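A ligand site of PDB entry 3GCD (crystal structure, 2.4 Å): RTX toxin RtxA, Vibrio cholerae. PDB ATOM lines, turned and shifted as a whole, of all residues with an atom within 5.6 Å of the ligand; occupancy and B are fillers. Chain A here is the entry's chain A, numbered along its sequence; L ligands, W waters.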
ATOM      1  N   LYS A   4       1.675  -7.134   4.350  1.00  0.00           N
ATOM      2  CA  LYS A   4       1.926  -6.325   3.119  1.00  0.00           C
ATOM      3  C   LYS A   4       0.910  -5.199   3.010  1.00  0.00           C
ATOM      4  O   LYS A   4      -0.193  -5.382   2.495  1.00  0.00           O
ATOM      5  CB  LYS A   4       1.856  -7.187   1.856  1.00  0.00           C
ATOM      6  CG  LYS A   4       3.109  -7.991   1.613  1.00  0.00           C
ATOM      7  CD  LYS A   4       4.320  -7.103   1.579  1.00  0.00           C
ATOM      8  CE  LYS A   4       5.605  -7.911   1.861  1.00  0.00           C
ATOM      9  NZ  LYS A   4       6.812  -7.022   1.877  1.00  0.00           N
ATOM     10  N   PRO A  42       8.479  -2.078  -0.357  1.00  0.00           N
ATOM     11  CA  PRO A  42       9.925  -2.300  -0.386  1.00  0.00           C
ATOM     12  C   PRO A  42      10.354  -3.478  -1.277  1.00  0.00           C
ATOM     13  O   PRO A  42      11.289  -3.333  -2.043  1.00  0.00           O
ATOM     14  CB  PRO A  42      10.265  -2.580   1.086  1.00  0.00           C
ATOM     15  CG  PRO A  42       9.192  -1.835   1.849  1.00  0.00           C
ATOM     16  CD  PRO A  42       7.942  -2.052   1.008  1.00  0.00           C
ATOM     17  N   VAL A  43       9.666  -4.616  -1.211  1.00  0.00           N
ATOM     18  CA  VAL A  43      10.036  -5.759  -2.057  1.00  0.00           C
ATOM     19  C   VAL A  43       9.817  -5.455  -3.558  1.00  0.00           C
ATOM     20  O   VAL A  43      10.692  -5.682  -4.386  1.00  0.00           O
ATOM     21  CB  VAL A  43       9.242  -7.052  -1.637  1.00  0.00           C
ATOM     22  CG1 VAL A  43       9.450  -8.177  -2.620  1.00  0.00           C
ATOM     23  CG2 VAL A  43       9.669  -7.485  -0.255  1.00  0.00           C
ATOM     24  N   VAL A  44       8.641  -4.937  -3.877  1.00  0.00           N
ATOM     25  CA  VAL A  44       8.284  -4.596  -5.241  1.00  0.00           C
ATOM     26  C   VAL A  44       9.260  -3.597  -5.821  1.00  0.00           C
ATOM     27  O   VAL A  44       9.615  -3.681  -7.002  1.00  0.00           O
ATOM     28  CB  VAL A  44       6.846  -4.043  -5.294  1.00  0.00           C
ATOM     29  CG1 VAL A  44       6.544  -3.413  -6.646  1.00  0.00           C
ATOM     30  CG2 VAL A  44       5.859  -5.170  -4.965  1.00  0.00           C
ATOM     31  N   LYS A  46      12.496  -3.124  -5.014  1.00  0.00           N
ATOM     32  CA  LYS A  46      13.775  -3.784  -5.286  1.00  0.00           C
ATOM     33  C   LYS A  46      13.697  -4.726  -6.469  1.00  0.00           C
ATOM     34  O   LYS A  46      14.631  -4.814  -7.253  1.00  0.00           O
ATOM     35  CB  LYS A  46      14.284  -4.533  -4.044  1.00  0.00           C
ATOM     36  CG  LYS A  46      15.089  -3.690  -3.042  1.00  0.00           C
ATOM     37  CD  LYS A  46      14.969  -4.298  -1.640  1.00  0.00           C
ATOM     38  CE  LYS A  46      15.657  -3.448  -0.589  1.00  0.00           C
ATOM     39  NZ  LYS A  46      15.032  -3.674   0.750  1.00  0.00           N
ATOM     40  N   ALA A  47      12.593  -5.454  -6.597  1.00  0.00           N
ATOM     41  CA  ALA A  47      12.415  -6.357  -7.740  1.00  0.00           C
ATOM     42  C   ALA A  47      12.358  -5.546  -9.030  1.00  0.00           C
ATOM     43  O   ALA A  47      12.910  -5.946 -10.068  1.00  0.00           O
ATOM     44  CB  ALA A  47      11.133  -7.180  -7.573  1.00  0.00           C
ATOM     45  N   ASN A  50      15.932  -4.449  -9.603  1.00  0.00           N
ATOM     46  CA  ASN A  50      16.754  -5.560 -10.025  1.00  0.00           C
ATOM     47  C   ASN A  50      16.509  -5.913 -11.482  1.00  0.00           C
ATOM     48  O   ASN A  50      17.454  -6.229 -12.191  1.00  0.00           O
ATOM     49  CB  ASN A  50      16.516  -6.787  -9.151  1.00  0.00           C
ATOM     50  CG  ASN A  50      17.068  -6.600  -7.734  1.00  0.00           C
ATOM     51  OD1 ASN A  50      17.682  -5.573  -7.414  1.00  0.00           O
ATOM     52  ND2 ASN A  50      16.845  -7.595  -6.891  1.00  0.00           N
ATOM     53  N   VAL A  89       5.382  -4.879 -12.066  1.00  0.00           N
ATOM     54  CA  VAL A  89       5.859  -5.450 -10.819  1.00  0.00           C
ATOM     55  C   VAL A  89       4.918  -5.083  -9.677  1.00  0.00           C
ATOM     56  O   VAL A  89       4.601  -3.907  -9.439  1.00  0.00           O
ATOM     57  CB  VAL A  89       7.300  -4.980 -10.505  1.00  0.00           C
ATOM     58  CG1 VAL A  89       7.836  -5.727  -9.331  1.00  0.00           C
ATOM     59  CG2 VAL A  89       8.210  -5.171 -11.752  1.00  0.00           C
ATOM     60  N   GLY A  90       4.460  -6.109  -8.977  1.00  0.00           N
ATOM     61  CA  GLY A  90       3.597  -5.895  -7.836  1.00  0.00           C
ATOM     62  C   GLY A  90       3.226  -7.161  -7.105  1.00  0.00           C
ATOM     63  O   GLY A  90       3.554  -8.271  -7.554  1.00  0.00           O
ATOM     64  N   HIS A  91       2.525  -7.009  -5.988  1.00  0.00           N
ATOM     65  CA  HIS A  91       2.079  -8.163  -5.245  1.00  0.00           C
ATOM     66  C   HIS A  91       0.734  -8.677  -5.780  1.00  0.00           C
ATOM     67  O   HIS A  91      -0.247  -7.939  -5.862  1.00  0.00           O
ATOM     68  CB  HIS A  91       1.968  -7.831  -3.752  1.00  0.00           C
ATOM     69  CG  HIS A  91       3.287  -7.750  -3.044  1.00  0.00           C
ATOM     70  ND1 HIS A  91       4.054  -8.871  -2.768  1.00  0.00           N
ATOM     71  CD2 HIS A  91       3.975  -6.701  -2.557  1.00  0.00           C
ATOM     72  CE1 HIS A  91       5.166  -8.504  -2.153  1.00  0.00           C
ATOM     73  NE2 HIS A  91       5.135  -7.195  -1.999  1.00  0.00           N
ATOM     74  N   GLY A  92       0.700  -9.958  -6.132  1.00  0.00           N
ATOM     75  CA  GLY A  92      -0.576 -10.610  -6.468  1.00  0.00           C
ATOM     76  C   GLY A  92      -1.239 -10.942  -5.132  1.00  0.00           C
ATOM     77  O   GLY A  92      -0.545 -11.383  -4.207  1.00  0.00           O
ATOM     78  N   ASN A 100      -4.816 -15.827  -7.814  1.00  0.00           N
ATOM     79  CA  ASN A 100      -5.005 -14.430  -7.384  1.00  0.00           C
ATOM     80  C   ASN A 100      -5.872 -13.627  -8.340  1.00  0.00           C
ATOM     81  O   ASN A 100      -5.882 -13.846  -9.554  1.00  0.00           O
ATOM     82  CB  ASN A 100      -3.670 -13.743  -7.193  1.00  0.00           C
ATOM     83  CG  ASN A 100      -3.013 -14.100  -5.871  1.00  0.00           C
ATOM     84  OD1 ASN A 100      -3.700 -14.249  -4.840  1.00  0.00           O
ATOM     85  ND2 ASN A 100      -1.684 -14.214  -5.873  1.00  0.00           N
ATOM     86  N   VAL A 138       4.869  -9.521 -13.342  1.00  0.00           N
ATOM     87  CA  VAL A 138       5.760 -10.007 -12.297  1.00  0.00           C
ATOM     88  C   VAL A 138       5.074  -9.907 -10.947  1.00  0.00           C
ATOM     89  O   VAL A 138       5.334  -8.993 -10.159  1.00  0.00           O
ATOM     90  CB  VAL A 138       7.126  -9.251 -12.305  1.00  0.00           C
ATOM     91  CG1 VAL A 138       8.051  -9.843 -11.266  1.00  0.00           C
ATOM     92  CG2 VAL A 138       7.783  -9.344 -13.678  1.00  0.00           C
ATOM     93  N   GLY A 139       4.173 -10.845 -10.702  1.00  0.00           N
ATOM     94  CA  GLY A 139       3.466 -10.931  -9.433  1.00  0.00           C
ATOM     95  C   GLY A 139       3.070 -12.385  -9.275  1.00  0.00           C
ATOM     96  O   GLY A 139       3.041 -13.115 -10.274  1.00  0.00           O
ATOM     97  N   CYS A 140       2.782 -12.805  -8.042  1.00  0.00           N
ATOM     98  CA  CYS A 140       2.507 -14.210  -7.722  1.00  0.00           C
ATOM     99  C   CYS A 140       1.209 -14.759  -8.272  1.00  0.00           C
ATOM    100  O   CYS A 140       0.136 -14.226  -7.989  1.00  0.00           O
ATOM    101  CB  CYS A 140       2.450 -14.426  -6.208  1.00  0.00           C
ATOM    102  SG  CYS A 140       4.068 -14.487  -5.369  1.00  0.00           S
ATOM    103  N   SER A 141       1.320 -15.841  -9.034  1.00  0.00           N
ATOM    104  CA  SER A 141       0.175 -16.592  -9.547  1.00  0.00           C
ATOM    105  C   SER A 141      -1.107 -15.909 -10.029  1.00  0.00           C
ATOM    106  O   SER A 141      -2.177 -16.063  -9.427  1.00  0.00           O
ATOM    107  CB  SER A 141      -0.225 -17.665  -8.550  1.00  0.00           C
ATOM    108  OG  SER A 141      -0.291 -17.121  -7.266  1.00  0.00           O
ATOM    109  N   GLU A 174       3.884 -19.182  -7.165  1.00  0.00           N
ATOM    110  CA  GLU A 174       4.614 -18.212  -6.382  1.00  0.00           C
ATOM    111  C   GLU A 174       5.768 -17.650  -7.222  1.00  0.00           C
ATOM    112  O   GLU A 174       6.356 -18.383  -8.012  1.00  0.00           O
ATOM    113  CB  GLU A 174       5.183 -18.882  -5.125  1.00  0.00           C
ATOM    114  CG  GLU A 174       5.234 -18.013  -3.884  1.00  0.00           C
ATOM    115  CD  GLU A 174       4.316 -18.500  -2.761  1.00  0.00           C
ATOM    116  OE1 GLU A 174       4.485 -18.041  -1.604  1.00  0.00           O
ATOM    117  OE2 GLU A 174       3.441 -19.335  -3.027  1.00  0.00           O
ATOM    118  N   LEU A 175       6.115 -16.386  -7.042  1.00  0.00           N
ATOM    119  CA  LEU A 175       7.147 -15.687  -7.834  1.00  0.00           C
ATOM    120  C   LEU A 175       8.112 -14.830  -7.048  1.00  0.00           C
ATOM    121  O   LEU A 175       7.747 -14.218  -6.105  1.00  0.00           O
ATOM    122  CB  LEU A 175       6.504 -14.861  -8.939  1.00  0.00           C
ATOM    123  CG  LEU A 175       7.299 -14.380 -10.144  1.00  0.00           C
ATOM    124  CD1 LEU A 175       6.593 -13.322 -10.876  1.00  0.00           C
ATOM    125  CD2 LEU A 175       8.528 -13.852  -9.701  1.00  0.00           C
ATOM    126  N   ALA A 176       9.331 -14.756  -7.514  1.00  0.00           N
ATOM    127  CA  ALA A 176      10.501 -14.298  -6.774  1.00  0.00           C
ATOM    128  C   ALA A 176      11.592 -13.797  -7.720  1.00  0.00           C
ATOM    129  O   ALA A 176      11.989 -14.506  -8.659  1.00  0.00           O
ATOM    130  CB  ALA A 176      11.038 -15.414  -5.897  1.00  0.00           C
ATOM    131  N   VAL A 177      12.070 -12.587  -7.476  1.00  0.00           N
ATOM    132  CA  VAL A 177      13.101 -11.999  -8.318  1.00  0.00           C
ATOM    133  C   VAL A 177      14.419 -11.886  -7.530  1.00  0.00           C
ATOM    134  O   VAL A 177      14.457 -11.264  -6.478  1.00  0.00           O
ATOM    135  CB  VAL A 177      12.692 -10.588  -8.794  1.00  0.00           C
ATOM    136  CG1 VAL A 177      13.755  -9.977  -9.683  1.00  0.00           C
ATOM    137  CG2 VAL A 177      11.337 -10.633  -9.496  1.00  0.00           C
ATOM    138  N   ASP A 178      15.493 -12.495  -8.053  1.00  0.00           N
ATOM    139  CA  ASP A 178      16.818 -12.414  -7.405  1.00  0.00           C
ATOM    140  C   ASP A 178      17.582 -11.132  -7.707  1.00  0.00           C
ATOM    141  O   ASP A 178      17.102 -10.268  -8.445  1.00  0.00           O
ATOM    142  CB  ASP A 178      17.685 -13.638  -7.730  1.00  0.00           C
ATOM    143  CG  ASP A 178      18.093 -13.692  -9.198  1.00  0.00           C
ATOM    144  OD1 ASP A 178      18.297 -12.625  -9.832  1.00  0.00           O
ATOM    145  OD2 ASP A 178      18.228 -14.826  -9.715  1.00  0.00           O
ATOM    146  N   GLU A 179      18.768 -11.018  -7.122  1.00  0.00           N
ATOM    147  CA  GLU A 179      19.527  -9.782  -7.213  1.00  0.00           C
ATOM    148  C   GLU A 179      20.004  -9.515  -8.637  1.00  0.00           C
ATOM    149  O   GLU A 179      20.355  -8.383  -8.977  1.00  0.00           O
ATOM    150  CB  GLU A 179      20.691  -9.803  -6.227  1.00  0.00           C
ATOM    151  CG  GLU A 179      21.525  -8.525  -6.191  1.00  0.00           C
ATOM    152  CD  GLU A 179      20.687  -7.234  -6.145  1.00  0.00           C
ATOM    153  OE1 GLU A 179      20.197  -6.781  -7.211  1.00  0.00           O
ATOM    154  OE2 GLU A 179      20.533  -6.663  -5.030  1.00  0.00           O
ATOM    155  N   HIS A 184      12.205 -16.562 -10.354  1.00  0.00           N
ATOM    156  CA  HIS A 184      12.157 -17.916  -9.822  1.00  0.00           C
ATOM    157  C   HIS A 184      10.726 -18.249  -9.463  1.00  0.00           C
ATOM    158  O   HIS A 184      10.034 -17.422  -8.865  1.00  0.00           O
ATOM    159  CB  HIS A 184      13.046 -18.045  -8.580  1.00  0.00           C
ATOM    160  CG  HIS A 184      14.464 -17.620  -8.811  1.00  0.00           C
ATOM    161  ND1 HIS A 184      15.515 -18.513  -8.841  1.00  0.00           N
ATOM    162  CD2 HIS A 184      15.005 -16.402  -9.033  1.00  0.00           C
ATOM    163  CE1 HIS A 184      16.641 -17.870  -9.051  1.00  0.00           C
ATOM    164  NE2 HIS A 184      16.365 -16.576  -9.172  1.00  0.00           N
ATOM    165  N   TRP A 192      12.190 -23.379  -4.687  1.00  0.00           N
ATOM    166  CA  TRP A 192      12.367 -22.415  -5.766  1.00  0.00           C
ATOM    167  C   TRP A 192      13.183 -22.998  -6.907  1.00  0.00           C
ATOM    168  O   TRP A 192      14.208 -23.637  -6.661  1.00  0.00           O
ATOM    169  CB  TRP A 192      13.017 -21.148  -5.265  1.00  0.00           C
ATOM    170  CG  TRP A 192      12.141 -20.386  -4.362  1.00  0.00           C
ATOM    171  CD1 TRP A 192      12.131 -20.429  -3.017  1.00  0.00           C
ATOM    172  CD2 TRP A 192      11.098 -19.481  -4.753  1.00  0.00           C
ATOM    173  NE1 TRP A 192      11.163 -19.596  -2.515  1.00  0.00           N
ATOM    174  CE2 TRP A 192      10.503 -19.002  -3.569  1.00  0.00           C
ATOM    175  CE3 TRP A 192      10.602 -19.023  -5.981  1.00  0.00           C
ATOM    176  CZ2 TRP A 192       9.452 -18.080  -3.579  1.00  0.00           C
ATOM    177  CZ3 TRP A 192       9.552 -18.120  -5.981  1.00  0.00           C
ATOM    178  CH2 TRP A 192       8.990 -17.658  -4.794  1.00  0.00           C
HETATM  179  C1  LIG L   1      13.365 -12.977  -2.907  1.00  0.00           C
HETATM  180  O1  LIG L   1      13.101 -13.200  -1.544  1.00  0.00           O
HETATM  181  O2  LIG L   1      14.115 -13.768  -3.520  1.00  0.00           O
HETATM  182  C2  LIG L   1      13.884 -15.174  -3.447  1.00  0.00           C
HETATM  183  C3  LIG L   1      15.027 -15.879  -4.154  1.00  0.00           C
HETATM  184  C4  LIG L   1      14.782 -17.013  -4.929  1.00  0.00           C
HETATM  185  C5  LIG L   1      15.842 -17.657  -5.574  1.00  0.00           C
HETATM  186  C6  LIG L   1      17.156 -17.186  -5.423  1.00  0.00           C
HETATM  187  C7  LIG L   1      17.400 -16.052  -4.638  1.00  0.00           C
HETATM  188  C8  LIG L   1      16.341 -15.398  -4.003  1.00  0.00           C
HETATM  189  N1  LIG L   1      13.291 -11.976  -3.719  1.00  0.00           N
HETATM  190  C9  LIG L   1      12.164 -11.008  -3.525  1.00  0.00           C
HETATM  191  C10 LIG L   1      10.821 -11.679  -3.878  1.00  0.00           C
HETATM  192  O3  LIG L   1      10.504 -11.893  -5.061  1.00  0.00           O
HETATM  193  C11 LIG L   1      12.412  -9.737  -4.349  1.00  0.00           C
HETATM  194  C12 LIG L   1      13.740  -9.048  -3.968  1.00  0.00           C
HETATM  195  C13 LIG L   1      14.417  -8.298  -5.137  1.00  0.00           C
HETATM  196  C14 LIG L   1      13.497  -8.114  -2.806  1.00  0.00           C
HETATM  197  N2  LIG L   1      10.038 -12.021  -2.854  1.00  0.00           N
HETATM  198  C15 LIG L   1       8.776 -12.729  -3.048  1.00  0.00           C
HETATM  199  C16 LIG L   1       7.670 -11.804  -3.556  1.00  0.00           C
HETATM  200  O4  LIG L   1       7.296 -10.826  -2.879  1.00  0.00           O
HETATM  201  C17 LIG L   1       8.349 -13.396  -1.746  1.00  0.00           C
HETATM  202  C18 LIG L   1       6.915 -13.926  -1.636  1.00  0.00           C
HETATM  203  C19 LIG L   1       6.659 -15.017  -2.674  1.00  0.00           C
HETATM  204  C20 LIG L   1       6.660 -14.419  -0.229  1.00  0.00           C
HETATM  205  O5  LIG L   1       1.289 -14.510  -3.335  1.00  0.00           O
HETATM  206  C21 LIG L   1       2.321 -14.065  -2.839  1.00  0.00           C
HETATM  207  O6  LIG L   1       2.966 -14.810  -1.754  1.00  0.00           O
HETATM  208  C22 LIG L   1       2.641 -14.537  -0.382  1.00  0.00           C
HETATM  209  C23 LIG L   1       2.896 -15.788   0.450  1.00  0.00           C
HETATM  210  C24 LIG L   1       2.910 -12.767  -3.348  1.00  0.00           C
HETATM  211  O7  LIG L   1       3.284 -11.963  -2.226  1.00  0.00           O
HETATM  212  C25 LIG L   1       4.115 -13.048  -4.285  1.00  0.00           C
HETATM  213  C26 LIG L   1       4.462 -11.785  -5.069  1.00  0.00           C
HETATM  214  O8  LIG L   1       3.559 -11.159  -5.624  1.00  0.00           O
HETATM  215  N3  LIG L   1       5.757 -11.401  -5.130  1.00  0.00           N
HETATM  216  N4  LIG L   1       6.686 -12.133  -4.500  1.00  0.00           N
HETATM  217  C27 LIG L   1       6.180 -10.177  -5.815  1.00  0.00           C
HETATM  218  C28 LIG L   1       7.374 -10.297  -6.735  1.00  0.00           C
HETATM  219  C29 LIG L   1       7.093 -11.272  -7.876  1.00  0.00           C
HETATM  220  C30 LIG L   1       7.693  -8.912  -7.281  1.00  0.00           C
HETATM  221  O   HOH W   1       7.031 -10.328   0.135  1.00  0.00           O
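An oxygen (O8) of the ligand sits close to the backbone carbonyl oxygen (O) of Gly 90. Residues that only touch the ligand: Val 43 (3.4 Å), Lys 46 (3.9 Å), Ala 47 (3.7 Å), Asn 50 (3.1 Å), Val 89 (3.8 Å), Asn 100 (3.9 Å), Val 138 (3.7 Å), Gly 139 (3.8 Å), Glu 174 (3.4 Å), Ala 176 (3.0 Å), Asp 178 (3.9 Å) and His 184 (3.4 Å). Of the 24 residues printed, 18 come within 4 Å of the ligand. The nearest printed residue that does not touch the ligand is Trp 192 (4.1 Å).
SG of Cys 140 is bonded to C25 of the ligand, 1.8 Å away. N of Gly 92 is in hydrogen-bond range of O8 of the ligand, 3.1 Å away. N of Cys 140 lies within hydrogen-bond range of O8 of the ligand (3.0 Å). A nitrogen (N1) of the ligand lies within hydrogen-bond range of the backbone carbonyl oxygen (O) of Val 177, 3.1 Å away. A ring nitrogen (ND1) of His 91 lies within hydrogen-bond range of an oxygen (O7) of the ligand (3.2 Å). The backbone carbonyl oxygen of Leu 175 lies within hydrogen-bond range of a nitrogen (N4) of the ligand, 2.8 Å away. The backbone NH of Val 177 sits at hydrogen-bond distance from an oxygen (O3) of the ligand (3.0 Å).
The backbone carbonyl oxygen (O) of Val 138 sits at hydrogen-bond distance from the backbone NH (N) of Gly 90 (3.2 Å). ND2 of Asn 100 lies within hydrogen-bond range of O of Cys 140. The backbone carbonyl oxygen (O) of Ala 176 sits at hydrogen-bond distance from the backbone NH (N) of His 184, 2.7 Å away. The backbone carbonyl oxygen (O) of Gly 92 lies close to the side-chain amide nitrogen (ND2) of Asn 100, at 3.5 Å. OD1 of Asn 50 sits close to OE1 of Glu 179, at 2.8 Å. A ring nitrogen (NE2) of His 184 sits at hydrogen-bond distance from the side-chain carboxylate (OD2) of Asp 178, at 2.6 Å. N of Asn 100 sits at hydrogen-bond distance from O of Ser 141, at 3.1 Å. The backbone NH of Leu 175 lies within hydrogen-bond range of the side-chain sulfur of Cys 140 (3.3 Å).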
